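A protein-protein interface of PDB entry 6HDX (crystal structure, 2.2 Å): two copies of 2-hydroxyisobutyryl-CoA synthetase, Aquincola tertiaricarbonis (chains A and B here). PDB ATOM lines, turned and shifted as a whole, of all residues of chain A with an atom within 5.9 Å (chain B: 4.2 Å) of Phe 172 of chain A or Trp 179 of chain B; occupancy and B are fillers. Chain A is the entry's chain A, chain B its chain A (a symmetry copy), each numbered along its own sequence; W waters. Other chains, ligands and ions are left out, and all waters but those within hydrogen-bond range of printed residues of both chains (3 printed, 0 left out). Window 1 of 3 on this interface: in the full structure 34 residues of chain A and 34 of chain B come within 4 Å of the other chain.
Phe 172 of chain B touches Phe 172 of chain A (CB to CB, 3.4 Å). CH2 of Trp 179 of chain B touches CD1 of Phe 172 of chain A, 3.9 Å away. Phe 195 of chain B touches Phe 172 of chain A (O to O, 3.9 Å). Phe 195 of chain B touches Leu 174 of chain A (CE2 to CD1, 3.8 Å). Phe 172 of chain B touches Trp 179 of chain A. Trp 179 of chain A touches Trp 179 of chain B. Trp 179 of chain A touches Leu 182 of chain B (CZ3 to CD2, 3.6 Å). His 125 of chain B touches Pro 194 of chain A (CE1 to CG, 3.7 Å). Pro 194 of chain A touches Ser 173 of chain B. O of Phe 195 of chain A touches O of Phe 172 of chain B (3.9 Å).
The backbone carbonyl oxygen (O) of Val 168 of chain A lies within hydrogen-bond range of the backbone NH (N) of Phe 195 of chain A, at 3.2 Å. NE1 of Trp 179 of chain A sits at hydrogen-bond distance from O of Ser 173 of chain A (2.8 Å). The backbone carbonyl oxygen (O) of Ser 173 of chain B lies within hydrogen-bond range of a ring nitrogen (ND1) of His 125 of chain B (3.1 Å). The indole nitrogen of Trp 179 of chain B lies within hydrogen-bond range of the backbone carbonyl oxygen of Ser 173 of chain B (2.8 Å).
Of the 16 printed residues of chain A, 7 touch a printed residue of chain B. Of the 15 printed residues of chain B, 6 touch a printed residue of chain A. Printed residues of chain B that touch a printed residue of chain A: His 125, Phe 172, Ser 173, Trp 179, Leu 182 and Phe 195. Among the printed residues, 14 pairs touch across the chains.
Water W2 lies within hydrogen-bond range of the backbone carbonyl oxygen of Phe 172 of chain B (2.8 Å), the backbone NH of Phe 172 of chain A (2.9 Å) and the backbone carbonyl oxygen of Ala 197 of chain A (3.3 Å). Water W3 lies within hydrogen-bond range of the backbone carbonyl oxygen of Phe 172 of chain A (2.8 Å) and the backbone NH of Phe 172 of chain B (2.9 Å). Water W1 lies within hydrogen-bond range of O of Pro 194 of chain A (3.3 Å), O of Ser 173 of chain B (3.3 Å) and ND1 of His 125 of chain B (3.4 Å).
Phe 172 of chain A touches three residues of chain B. Of chain A, only Phe 172, Trp 179, Leu 182 and Pro 194 come within 4 Å of Trp 179 of chain B. Printed residues of chain B within 4 Å of Leu 182 of chain A: Trp 179. Printed residues of chain B within 4 Å of Pro 194 of chain A: His 125, Ser 173 and Trp 179. Of the printed residues of chain B, Ser 173 of chain A touches Phe 195. Ser 178 of chain B touches none of the printed residues of chain A. Ala 197 of chain A touches none of the printed residues of chain B. The nearest printed residue of chain A that does not touch Ser 173 of chain B is Gly 196 of chain A (4.8 Å).
The side-chain hydroxyl of Ser 173 of chain A is in hydrogen-bond range of the backbone carbonyl oxygen of Phe 195 of chain B, at 2.6 Å. The side-chain hydroxyl of Ser 173 of chain B sits at hydrogen-bond distance from the backbone carbonyl oxygen of Phe 195 of chain A, at 2.6 Å.
Phe 172 of chain B touches its own counterpart, Phe 172 of chain A. Phe 172 of chain A touches Phe 195 of chain B, and with the chains exchanged Phe 195 of chain A touches Phe 172 of chain B. Ser 173 of chain A touches Phe 195 of chain B, and with the chains exchanged Phe 195 of chain A touches Ser 173 of chain B. Trp 179 of chain A touches Leu 182 of chain B, and with the chains exchanged Leu 182 of chain A touches Trp 179 of chain B. Of the 14 pairs that touch across the chains among the printed residues, 10 have their exchanged pair printed and touching as well.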
ATOM      1  N   VAL A 168     -21.348  18.722  33.370  1.00  0.00           N
ATOM      2  CA  VAL A 168     -20.845  19.762  32.450  1.00  0.00           C
ATOM      3  C   VAL A 168     -21.506  21.082  32.888  1.00  0.00           C
ATOM      4  O   VAL A 168     -22.695  21.312  32.650  1.00  0.00           O
ATOM      5  CB  VAL A 168     -21.034  19.434  30.934  1.00  0.00           C
ATOM      6  CG1 VAL A 168     -20.451  20.545  30.051  1.00  0.00           C
ATOM      7  CG2 VAL A 168     -20.382  18.103  30.592  1.00  0.00           C
ATOM      8  N   ALA A 169     -20.733  21.901  33.608  1.00  0.00           N
ATOM      9  CA  ALA A 169     -21.208  23.137  34.215  1.00  0.00           C
ATOM     10  C   ALA A 169     -20.564  24.405  33.660  1.00  0.00           C
ATOM     11  O   ALA A 169     -19.960  25.192  34.394  1.00  0.00           O
ATOM     12  CB  ALA A 169     -21.056  23.056  35.728  1.00  0.00           C
ATOM     13  N   ALA A 170     -20.702  24.602  32.358  1.00  0.00           N
ATOM     14  CA  ALA A 170     -20.318  25.841  31.652  1.00  0.00           C
ATOM     15  C   ALA A 170     -21.518  26.150  30.728  1.00  0.00           C
ATOM     16  O   ALA A 170     -22.279  25.232  30.380  1.00  0.00           O
ATOM     17  CB  ALA A 170     -19.040  25.645  30.839  1.00  0.00           C
ATOM     18  N   VAL A 171     -21.713  27.423  30.384  1.00  0.00           N
ATOM     19  CA  VAL A 171     -22.813  27.888  29.556  1.00  0.00           C
ATOM     20  C   VAL A 171     -22.923  27.101  28.207  1.00  0.00           C
ATOM     21  O   VAL A 171     -21.930  26.912  27.527  1.00  0.00           O
ATOM     22  CB  VAL A 171     -22.772  29.438  29.361  1.00  0.00           C
ATOM     23  CG1 VAL A 171     -21.534  29.884  28.568  1.00  0.00           C
ATOM     24  CG2 VAL A 171     -24.049  29.951  28.694  1.00  0.00           C
ATOM     25  N   PHE A 172     -24.131  26.620  27.860  1.00  0.00           N
ATOM     26  CA  PHE A 172     -24.389  25.954  26.576  1.00  0.00           C
ATOM     27  C   PHE A 172     -25.031  26.988  25.673  1.00  0.00           C
ATOM     28  O   PHE A 172     -26.209  27.310  25.825  1.00  0.00           O
ATOM     29  CB  PHE A 172     -25.292  24.732  26.744  1.00  0.00           C
ATOM     30  CG  PHE A 172     -24.601  23.530  27.316  1.00  0.00           C
ATOM     31  CD1 PHE A 172     -23.972  22.610  26.484  1.00  0.00           C
ATOM     32  CD2 PHE A 172     -24.589  23.305  28.688  1.00  0.00           C
ATOM     33  CE1 PHE A 172     -23.313  21.508  27.021  1.00  0.00           C
ATOM     34  CE2 PHE A 172     -23.924  22.202  29.226  1.00  0.00           C
ATOM     35  CZ  PHE A 172     -23.302  21.307  28.390  1.00  0.00           C
ATOM     36  N   SER A 173     -24.211  27.603  24.826  1.00  0.00           N
ATOM     37  CA  SER A 173     -24.613  28.677  23.911  1.00  0.00           C
ATOM     38  C   SER A 173     -23.597  28.684  22.769  1.00  0.00           C
ATOM     39  O   SER A 173     -23.243  27.612  22.281  1.00  0.00           O
ATOM     40  CB  SER A 173     -24.636  30.024  24.648  1.00  0.00           C
ATOM     41  OG  SER A 173     -25.058  31.092  23.805  1.00  0.00           O
ATOM     42  N   LEU A 174     -23.083  29.869  22.380  1.00  0.00           N
ATOM     43  CA  LEU A 174     -22.062  30.014  21.328  1.00  0.00           C
ATOM     44  C   LEU A 174     -20.753  29.321  21.725  1.00  0.00           C
ATOM     45  O   LEU A 174     -20.067  28.772  20.875  1.00  0.00           O
ATOM     46  CB  LEU A 174     -21.784  31.517  21.105  1.00  0.00           C
ATOM     47  CG  LEU A 174     -22.865  32.342  20.395  1.00  0.00           C
ATOM     48  CD1 LEU A 174     -22.505  33.780  20.426  1.00  0.00           C
ATOM     49  CD2 LEU A 174     -23.054  31.892  18.940  1.00  0.00           C
ATOM     50  N   TYR A 175     -20.417  29.357  23.015  1.00  0.00           N
ATOM     51  CA  TYR A 175     -19.189  28.841  23.629  1.00  0.00           C
ATOM     52  C   TYR A 175     -18.950  27.338  23.399  1.00  0.00           C
ATOM     53  O   TYR A 175     -19.796  26.511  23.757  1.00  0.00           O
ATOM     54  CB  TYR A 175     -19.197  29.198  25.119  1.00  0.00           C
ATOM     55  CG  TYR A 175     -17.956  28.766  25.867  1.00  0.00           C
ATOM     56  CD1 TYR A 175     -16.699  29.263  25.520  1.00  0.00           C
ATOM     57  CD2 TYR A 175     -18.040  27.906  26.957  1.00  0.00           C
ATOM     58  CE1 TYR A 175     -15.557  28.905  26.236  1.00  0.00           C
ATOM     59  CE2 TYR A 175     -16.908  27.553  27.688  1.00  0.00           C
ATOM     60  CZ  TYR A 175     -15.668  28.049  27.318  1.00  0.00           C
ATOM     61  OH  TYR A 175     -14.551  27.713  28.025  1.00  0.00           O
ATOM     62  N   SER A 178     -18.363  23.941  26.765  1.00  0.00           N
ATOM     63  CA  SER A 178     -19.439  23.102  27.296  1.00  0.00           C
ATOM     64  C   SER A 178     -19.824  21.975  26.312  1.00  0.00           C
ATOM     65  O   SER A 178     -19.854  20.808  26.713  1.00  0.00           O
ATOM     66  CB  SER A 178     -20.652  23.967  27.598  1.00  0.00           C
ATOM     67  OG  SER A 178     -20.998  24.678  26.418  1.00  0.00           O
ATOM     68  N   TRP A 179     -20.076  22.328  25.026  1.00  0.00           N
ATOM     69  CA  TRP A 179     -20.455  21.383  23.963  1.00  0.00           C
ATOM     70  C   TRP A 179     -19.375  20.338  23.770  1.00  0.00           C
ATOM     71  O   TRP A 179     -19.687  19.160  23.649  1.00  0.00           O
ATOM     72  CB  TRP A 179     -20.774  22.105  22.615  1.00  0.00           C
ATOM     73  CG  TRP A 179     -21.932  23.055  22.725  1.00  0.00           C
ATOM     74  CD1 TRP A 179     -21.865  24.402  22.910  1.00  0.00           C
ATOM     75  CD2 TRP A 179     -23.325  22.702  22.817  1.00  0.00           C
ATOM     76  NE1 TRP A 179     -23.130  24.923  23.065  1.00  0.00           N
ATOM     77  CE2 TRP A 179     -24.046  23.899  23.018  1.00  0.00           C
ATOM     78  CE3 TRP A 179     -24.031  21.482  22.776  1.00  0.00           C
ATOM     79  CZ2 TRP A 179     -25.451  23.924  23.141  1.00  0.00           C
ATOM     80  CZ3 TRP A 179     -25.420  21.501  22.901  1.00  0.00           C
ATOM     81  CH2 TRP A 179     -26.117  22.709  23.057  1.00  0.00           C
ATOM     82  N   LEU A 182     -19.367  17.856  26.755  1.00  0.00           N
ATOM     83  CA  LEU A 182     -20.577  17.042  26.622  1.00  0.00           C
ATOM     84  C   LEU A 182     -20.402  15.944  25.525  1.00  0.00           C
ATOM     85  O   LEU A 182     -20.726  14.772  25.770  1.00  0.00           O
ATOM     86  CB  LEU A 182     -21.770  17.946  26.276  1.00  0.00           C
ATOM     87  CG  LEU A 182     -23.083  17.252  25.897  1.00  0.00           C
ATOM     88  CD1 LEU A 182     -23.660  16.467  27.085  1.00  0.00           C
ATOM     89  CD2 LEU A 182     -24.094  18.258  25.393  1.00  0.00           C
ATOM     90  N   GLU A 186     -20.616  11.947  26.183  1.00  0.00           N
ATOM     91  CA  GLU A 186     -21.548  11.131  25.396  1.00  0.00           C
ATOM     92  C   GLU A 186     -20.831   9.946  24.742  1.00  0.00           C
ATOM     93  O   GLU A 186     -21.280   8.803  24.895  1.00  0.00           O
ATOM     94  CB  GLU A 186     -22.213  11.991  24.307  1.00  0.00           C
ATOM     95  CG  GLU A 186     -23.293  12.950  24.822  1.00  0.00           C
ATOM     96  CD  GLU A 186     -23.863  13.928  23.807  1.00  0.00           C
ATOM     97  OE1 GLU A 186     -23.294  14.062  22.704  1.00  0.00           O
ATOM     98  OE2 GLU A 186     -24.868  14.594  24.129  1.00  0.00           O
ATOM     99  N   PRO A 194     -25.527  17.604  31.519  1.00  0.00           N
ATOM    100  CA  PRO A 194     -25.289  18.992  31.082  1.00  0.00           C
ATOM    101  C   PRO A 194     -26.143  20.030  31.813  1.00  0.00           C
ATOM    102  O   PRO A 194     -27.131  20.541  31.288  1.00  0.00           O
ATOM    103  CB  PRO A 194     -25.540  18.929  29.578  1.00  0.00           C
ATOM    104  CG  PRO A 194     -26.538  17.799  29.392  1.00  0.00           C
ATOM    105  CD  PRO A 194     -26.451  16.900  30.595  1.00  0.00           C
ATOM    106  N   PHE A 195     -25.730  20.351  33.046  1.00  0.00           N
ATOM    107  CA  PHE A 195     -26.406  21.344  33.878  1.00  0.00           C
ATOM    108  C   PHE A 195     -26.194  22.736  33.297  1.00  0.00           C
ATOM    109  O   PHE A 195     -27.085  23.548  33.383  1.00  0.00           O
ATOM    110  CB  PHE A 195     -25.944  21.280  35.364  1.00  0.00           C
ATOM    111  CG  PHE A 195     -26.770  22.141  36.310  1.00  0.00           C
ATOM    112  CD1 PHE A 195     -26.436  23.479  36.535  1.00  0.00           C
ATOM    113  CD2 PHE A 195     -27.871  21.611  36.980  1.00  0.00           C
ATOM    114  CE1 PHE A 195     -27.201  24.276  37.391  1.00  0.00           C
ATOM    115  CE2 PHE A 195     -28.663  22.423  37.804  1.00  0.00           C
ATOM    116  CZ  PHE A 195     -28.321  23.754  38.005  1.00  0.00           C
ATOM    117  N   GLY A 196     -25.039  23.012  32.711  1.00  0.00           N
ATOM    118  CA  GLY A 196     -24.816  24.337  32.141  1.00  0.00           C
ATOM    119  C   GLY A 196     -24.530  25.404  33.162  1.00  0.00           C
ATOM    120  O   GLY A 196     -24.171  25.104  34.304  1.00  0.00           O
ATOM    121  N   ALA A 197     -24.647  26.675  32.750  1.00  0.00           N
ATOM    122  CA  ALA A 197     -24.339  27.831  33.614  1.00  0.00           C
ATOM    123  C   ALA A 197     -24.873  29.084  32.965  1.00  0.00           C
ATOM    124  O   ALA A 197     -25.367  29.008  31.851  1.00  0.00           O
ATOM    125  CB  ALA A 197     -22.827  27.953  33.803  1.00  0.00           C
ATOM    126  N   HIS B 125     -31.062  14.971  33.166  1.00  0.00           N
ATOM    127  CA  HIS B 125     -31.772  16.248  33.179  1.00  0.00           C
ATOM    128  C   HIS B 125     -32.752  16.190  34.344  1.00  0.00           C
ATOM    129  O   HIS B 125     -32.654  15.295  35.175  1.00  0.00           O
ATOM    130  CB  HIS B 125     -32.500  16.494  31.838  1.00  0.00           C
ATOM    131  CG  HIS B 125     -31.588  16.569  30.658  1.00  0.00           C
ATOM    132  ND1 HIS B 125     -30.977  17.754  30.295  1.00  0.00           N
ATOM    133  CD2 HIS B 125     -31.187  15.584  29.812  1.00  0.00           C
ATOM    134  CE1 HIS B 125     -30.207  17.452  29.260  1.00  0.00           C
ATOM    135  NE2 HIS B 125     -30.324  16.168  28.912  1.00  0.00           N
ATOM    136  N   TRP B 144     -32.874   8.488  23.740  1.00  0.00           N
ATOM    137  CA  TRP B 144     -32.399   9.762  23.193  1.00  0.00           C
ATOM    138  C   TRP B 144     -32.540   9.736  21.648  1.00  0.00           C
ATOM    139  O   TRP B 144     -33.001  10.715  21.053  1.00  0.00           O
ATOM    140  CB  TRP B 144     -30.947  10.080  23.662  1.00  0.00           C
ATOM    141  CG  TRP B 144     -30.587  11.522  23.488  1.00  0.00           C
ATOM    142  CD1 TRP B 144     -30.053  12.100  22.374  1.00  0.00           C
ATOM    143  CD2 TRP B 144     -30.907  12.602  24.389  1.00  0.00           C
ATOM    144  NE1 TRP B 144     -29.981  13.470  22.538  1.00  0.00           N
ATOM    145  CE2 TRP B 144     -30.470  13.800  23.778  1.00  0.00           C
ATOM    146  CE3 TRP B 144     -31.494  12.667  25.668  1.00  0.00           C
ATOM    147  CZ2 TRP B 144     -30.604  15.051  24.400  1.00  0.00           C
ATOM    148  CZ3 TRP B 144     -31.611  13.907  26.291  1.00  0.00           C
ATOM    149  CH2 TRP B 144     -31.173  15.080  25.659  1.00  0.00           C
ATOM    150  N   PHE B 172     -30.264  25.689  28.036  1.00  0.00           N
ATOM    151  CA  PHE B 172     -29.736  24.320  27.956  1.00  0.00           C
ATOM    152  C   PHE B 172     -29.187  23.986  29.329  1.00  0.00           C
ATOM    153  O   PHE B 172     -28.113  24.455  29.706  1.00  0.00           O
ATOM    154  CB  PHE B 172     -28.654  24.193  26.884  1.00  0.00           C
ATOM    155  CG  PHE B 172     -29.181  24.154  25.479  1.00  0.00           C
ATOM    156  CD1 PHE B 172     -29.527  22.947  24.885  1.00  0.00           C
ATOM    157  CD2 PHE B 172     -29.318  25.325  24.741  1.00  0.00           C
ATOM    158  CE1 PHE B 172     -30.037  22.918  23.589  1.00  0.00           C
ATOM    159  CE2 PHE B 172     -29.834  25.296  23.444  1.00  0.00           C
ATOM    160  CZ  PHE B 172     -30.177  24.094  22.874  1.00  0.00           C
ATOM    161  N   SER B 173     -29.996  23.287  30.119  1.00  0.00           N
ATOM    162  CA  SER B 173     -29.687  22.913  31.503  1.00  0.00           C
ATOM    163  C   SER B 173     -30.541  21.688  31.828  1.00  0.00           C
ATOM    164  O   SER B 173     -30.633  20.789  30.995  1.00  0.00           O
ATOM    165  CB  SER B 173     -29.997  24.080  32.452  1.00  0.00           C
ATOM    166  OG  SER B 173     -29.676  23.773  33.806  1.00  0.00           O
ATOM    167  N   TYR B 175     -33.796  21.583  31.964  1.00  0.00           N
ATOM    168  CA  TYR B 175     -34.977  21.735  31.105  1.00  0.00           C
ATOM    169  C   TYR B 175     -34.910  20.935  29.792  1.00  0.00           C
ATOM    170  O   TYR B 175     -33.978  21.115  29.000  1.00  0.00           O
ATOM    171  CB  TYR B 175     -35.213  23.227  30.856  1.00  0.00           C
ATOM    172  CG  TYR B 175     -36.438  23.530  30.021  1.00  0.00           C
ATOM    173  CD1 TYR B 175     -37.712  23.166  30.457  1.00  0.00           C
ATOM    174  CD2 TYR B 175     -36.332  24.229  28.823  1.00  0.00           C
ATOM    175  CE1 TYR B 175     -38.849  23.484  29.715  1.00  0.00           C
ATOM    176  CE2 TYR B 175     -37.462  24.565  28.080  1.00  0.00           C
ATOM    177  CZ  TYR B 175     -38.717  24.183  28.527  1.00  0.00           C
ATOM    178  OH  TYR B 175     -39.832  24.505  27.811  1.00  0.00           O
ATOM    179  N   MET B 176     -35.924  20.072  29.551  1.00  0.00           N
ATOM    180  CA  MET B 176     -35.943  19.189  28.375  1.00  0.00           C
ATOM    181  C   MET B 176     -36.254  19.850  27.048  1.00  0.00           C
ATOM    182  O   MET B 176     -35.876  19.293  26.006  1.00  0.00           O
ATOM    183  CB  MET B 176     -36.889  17.996  28.577  1.00  0.00           C
ATOM    184  CG  MET B 176     -36.352  16.943  29.567  1.00  0.00           C
ATOM    185  SD  MET B 176     -34.768  16.209  29.106  1.00  0.00           S
ATOM    186  CE  MET B 176     -35.175  15.389  27.547  1.00  0.00           C
ATOM    187  N   GLY B 177     -36.970  20.976  27.082  1.00  0.00           N
ATOM    188  CA  GLY B 177     -37.403  21.699  25.901  1.00  0.00           C
ATOM    189  C   GLY B 177     -36.335  21.979  24.876  1.00  0.00           C
ATOM    190  O   GLY B 177     -36.478  21.617  23.702  1.00  0.00           O
ATOM    191  N   SER B 178     -35.277  22.673  25.312  1.00  0.00           N
ATOM    192  CA  SER B 178     -34.140  23.048  24.471  1.00  0.00           C
ATOM    193  C   SER B 178     -33.441  21.809  23.867  1.00  0.00           C
ATOM    194  O   SER B 178     -33.249  21.757  22.649  1.00  0.00           O
ATOM    195  CB  SER B 178     -33.148  23.857  25.291  1.00  0.00           C
ATOM    196  OG  SER B 178     -32.796  23.099  26.440  1.00  0.00           O
ATOM    197  N   TRP B 179     -33.103  20.807  24.719  1.00  0.00           N
ATOM    198  CA  TRP B 179     -32.433  19.561  24.312  1.00  0.00           C
ATOM    199  C   TRP B 179     -33.275  18.809  23.301  1.00  0.00           C
ATOM    200  O   TRP B 179     -32.743  18.328  22.309  1.00  0.00           O
ATOM    201  CB  TRP B 179     -32.089  18.648  25.533  1.00  0.00           C
ATOM    202  CG  TRP B 179     -31.144  19.303  26.498  1.00  0.00           C
ATOM    203  CD1 TRP B 179     -31.475  19.950  27.651  1.00  0.00           C
ATOM    204  CD2 TRP B 179     -29.731  19.511  26.309  1.00  0.00           C
ATOM    205  NE1 TRP B 179     -30.353  20.508  28.220  1.00  0.00           N
ATOM    206  CE2 TRP B 179     -29.268  20.260  27.413  1.00  0.00           C
ATOM    207  CE3 TRP B 179     -28.816  19.158  25.295  1.00  0.00           C
ATOM    208  CZ2 TRP B 179     -27.916  20.635  27.558  1.00  0.00           C
ATOM    209  CZ3 TRP B 179     -27.480  19.530  25.433  1.00  0.00           C
ATOM    210  CH2 TRP B 179     -27.036  20.237  26.561  1.00  0.00           C
ATOM    211  N   GLY B 180     -34.579  18.752  23.541  1.00  0.00           N
ATOM    212  CA  GLY B 180     -35.532  18.102  22.638  1.00  0.00           C
ATOM    213  C   GLY B 180     -35.606  18.700  21.248  1.00  0.00           C
ATOM    214  O   GLY B 180     -35.684  17.969  20.270  1.00  0.00           O
ATOM    215  N   ALA B 181     -35.604  20.029  21.139  1.00  0.00           N
ATOM    216  CA  ALA B 181     -35.657  20.729  19.845  1.00  0.00           C
ATOM    217  C   ALA B 181     -34.301  20.592  19.112  1.00  0.00           C
ATOM    218  O   ALA B 181     -34.261  20.447  17.886  1.00  0.00           O
ATOM    219  CB  ALA B 181     -36.004  22.196  20.061  1.00  0.00           C
ATOM    220  N   LEU B 182     -33.196  20.635  19.876  1.00  0.00           N
ATOM    221  CA  LEU B 182     -31.852  20.437  19.330  1.00  0.00           C
ATOM    222  C   LEU B 182     -31.692  19.004  18.730  1.00  0.00           C
ATOM    223  O   LEU B 182     -31.193  18.861  17.603  1.00  0.00           O
ATOM    224  CB  LEU B 182     -30.809  20.664  20.435  1.00  0.00           C
ATOM    225  CG  LEU B 182     -29.356  20.303  20.106  1.00  0.00           C
ATOM    226  CD1 LEU B 182     -28.796  21.209  18.999  1.00  0.00           C
ATOM    227  CD2 LEU B 182     -28.490  20.391  21.343  1.00  0.00           C
ATOM    228  N   ALA B 183     -32.085  17.953  19.499  1.00  0.00           N
ATOM    229  CA  ALA B 183     -31.988  16.547  19.050  1.00  0.00           C
ATOM    230  C   ALA B 183     -32.771  16.321  17.748  1.00  0.00           C
ATOM    231  O   ALA B 183     -32.310  15.577  16.886  1.00  0.00           O
ATOM    232  CB  ALA B 183     -32.451  15.584  20.148  1.00  0.00           C
ATOM    233  N   PHE B 195     -28.199  28.441  20.492  1.00  0.00           N
ATOM    234  CA  PHE B 195     -27.819  29.685  21.160  1.00  0.00           C
ATOM    235  C   PHE B 195     -28.207  29.621  22.632  1.00  0.00           C
ATOM    236  O   PHE B 195     -27.495  30.155  23.449  1.00  0.00           O
ATOM    237  CB  PHE B 195     -28.439  30.937  20.470  1.00  0.00           C
ATOM    238  CG  PHE B 195     -27.903  32.262  20.991  1.00  0.00           C
ATOM    239  CD1 PHE B 195     -28.498  32.895  22.087  1.00  0.00           C
ATOM    240  CD2 PHE B 195     -26.814  32.882  20.381  1.00  0.00           C
ATOM    241  CE1 PHE B 195     -27.999  34.105  22.577  1.00  0.00           C
ATOM    242  CE2 PHE B 195     -26.287  34.073  20.900  1.00  0.00           C
ATOM    243  CZ  PHE B 195     -26.885  34.678  21.998  1.00  0.00           C
ATOM    244  N   GLY B 196     -29.314  28.977  22.971  1.00  0.00           N
ATOM    245  CA  GLY B 196     -29.702  28.897  24.375  1.00  0.00           C
ATOM    246  C   GLY B 196     -30.297  30.165  24.921  1.00  0.00           C
ATOM    247  O   GLY B 196     -30.731  31.036  24.161  1.00  0.00           O
HETATM  248  O   HOH W   1     -29.117  18.576  32.980  1.00  0.00           O
HETATM  249  O   HOH W   2     -26.212  26.544  29.873  1.00  0.00           O
HETATM  250  O   HOH W   3     -28.463  27.877  27.440  1.00  0.00           O
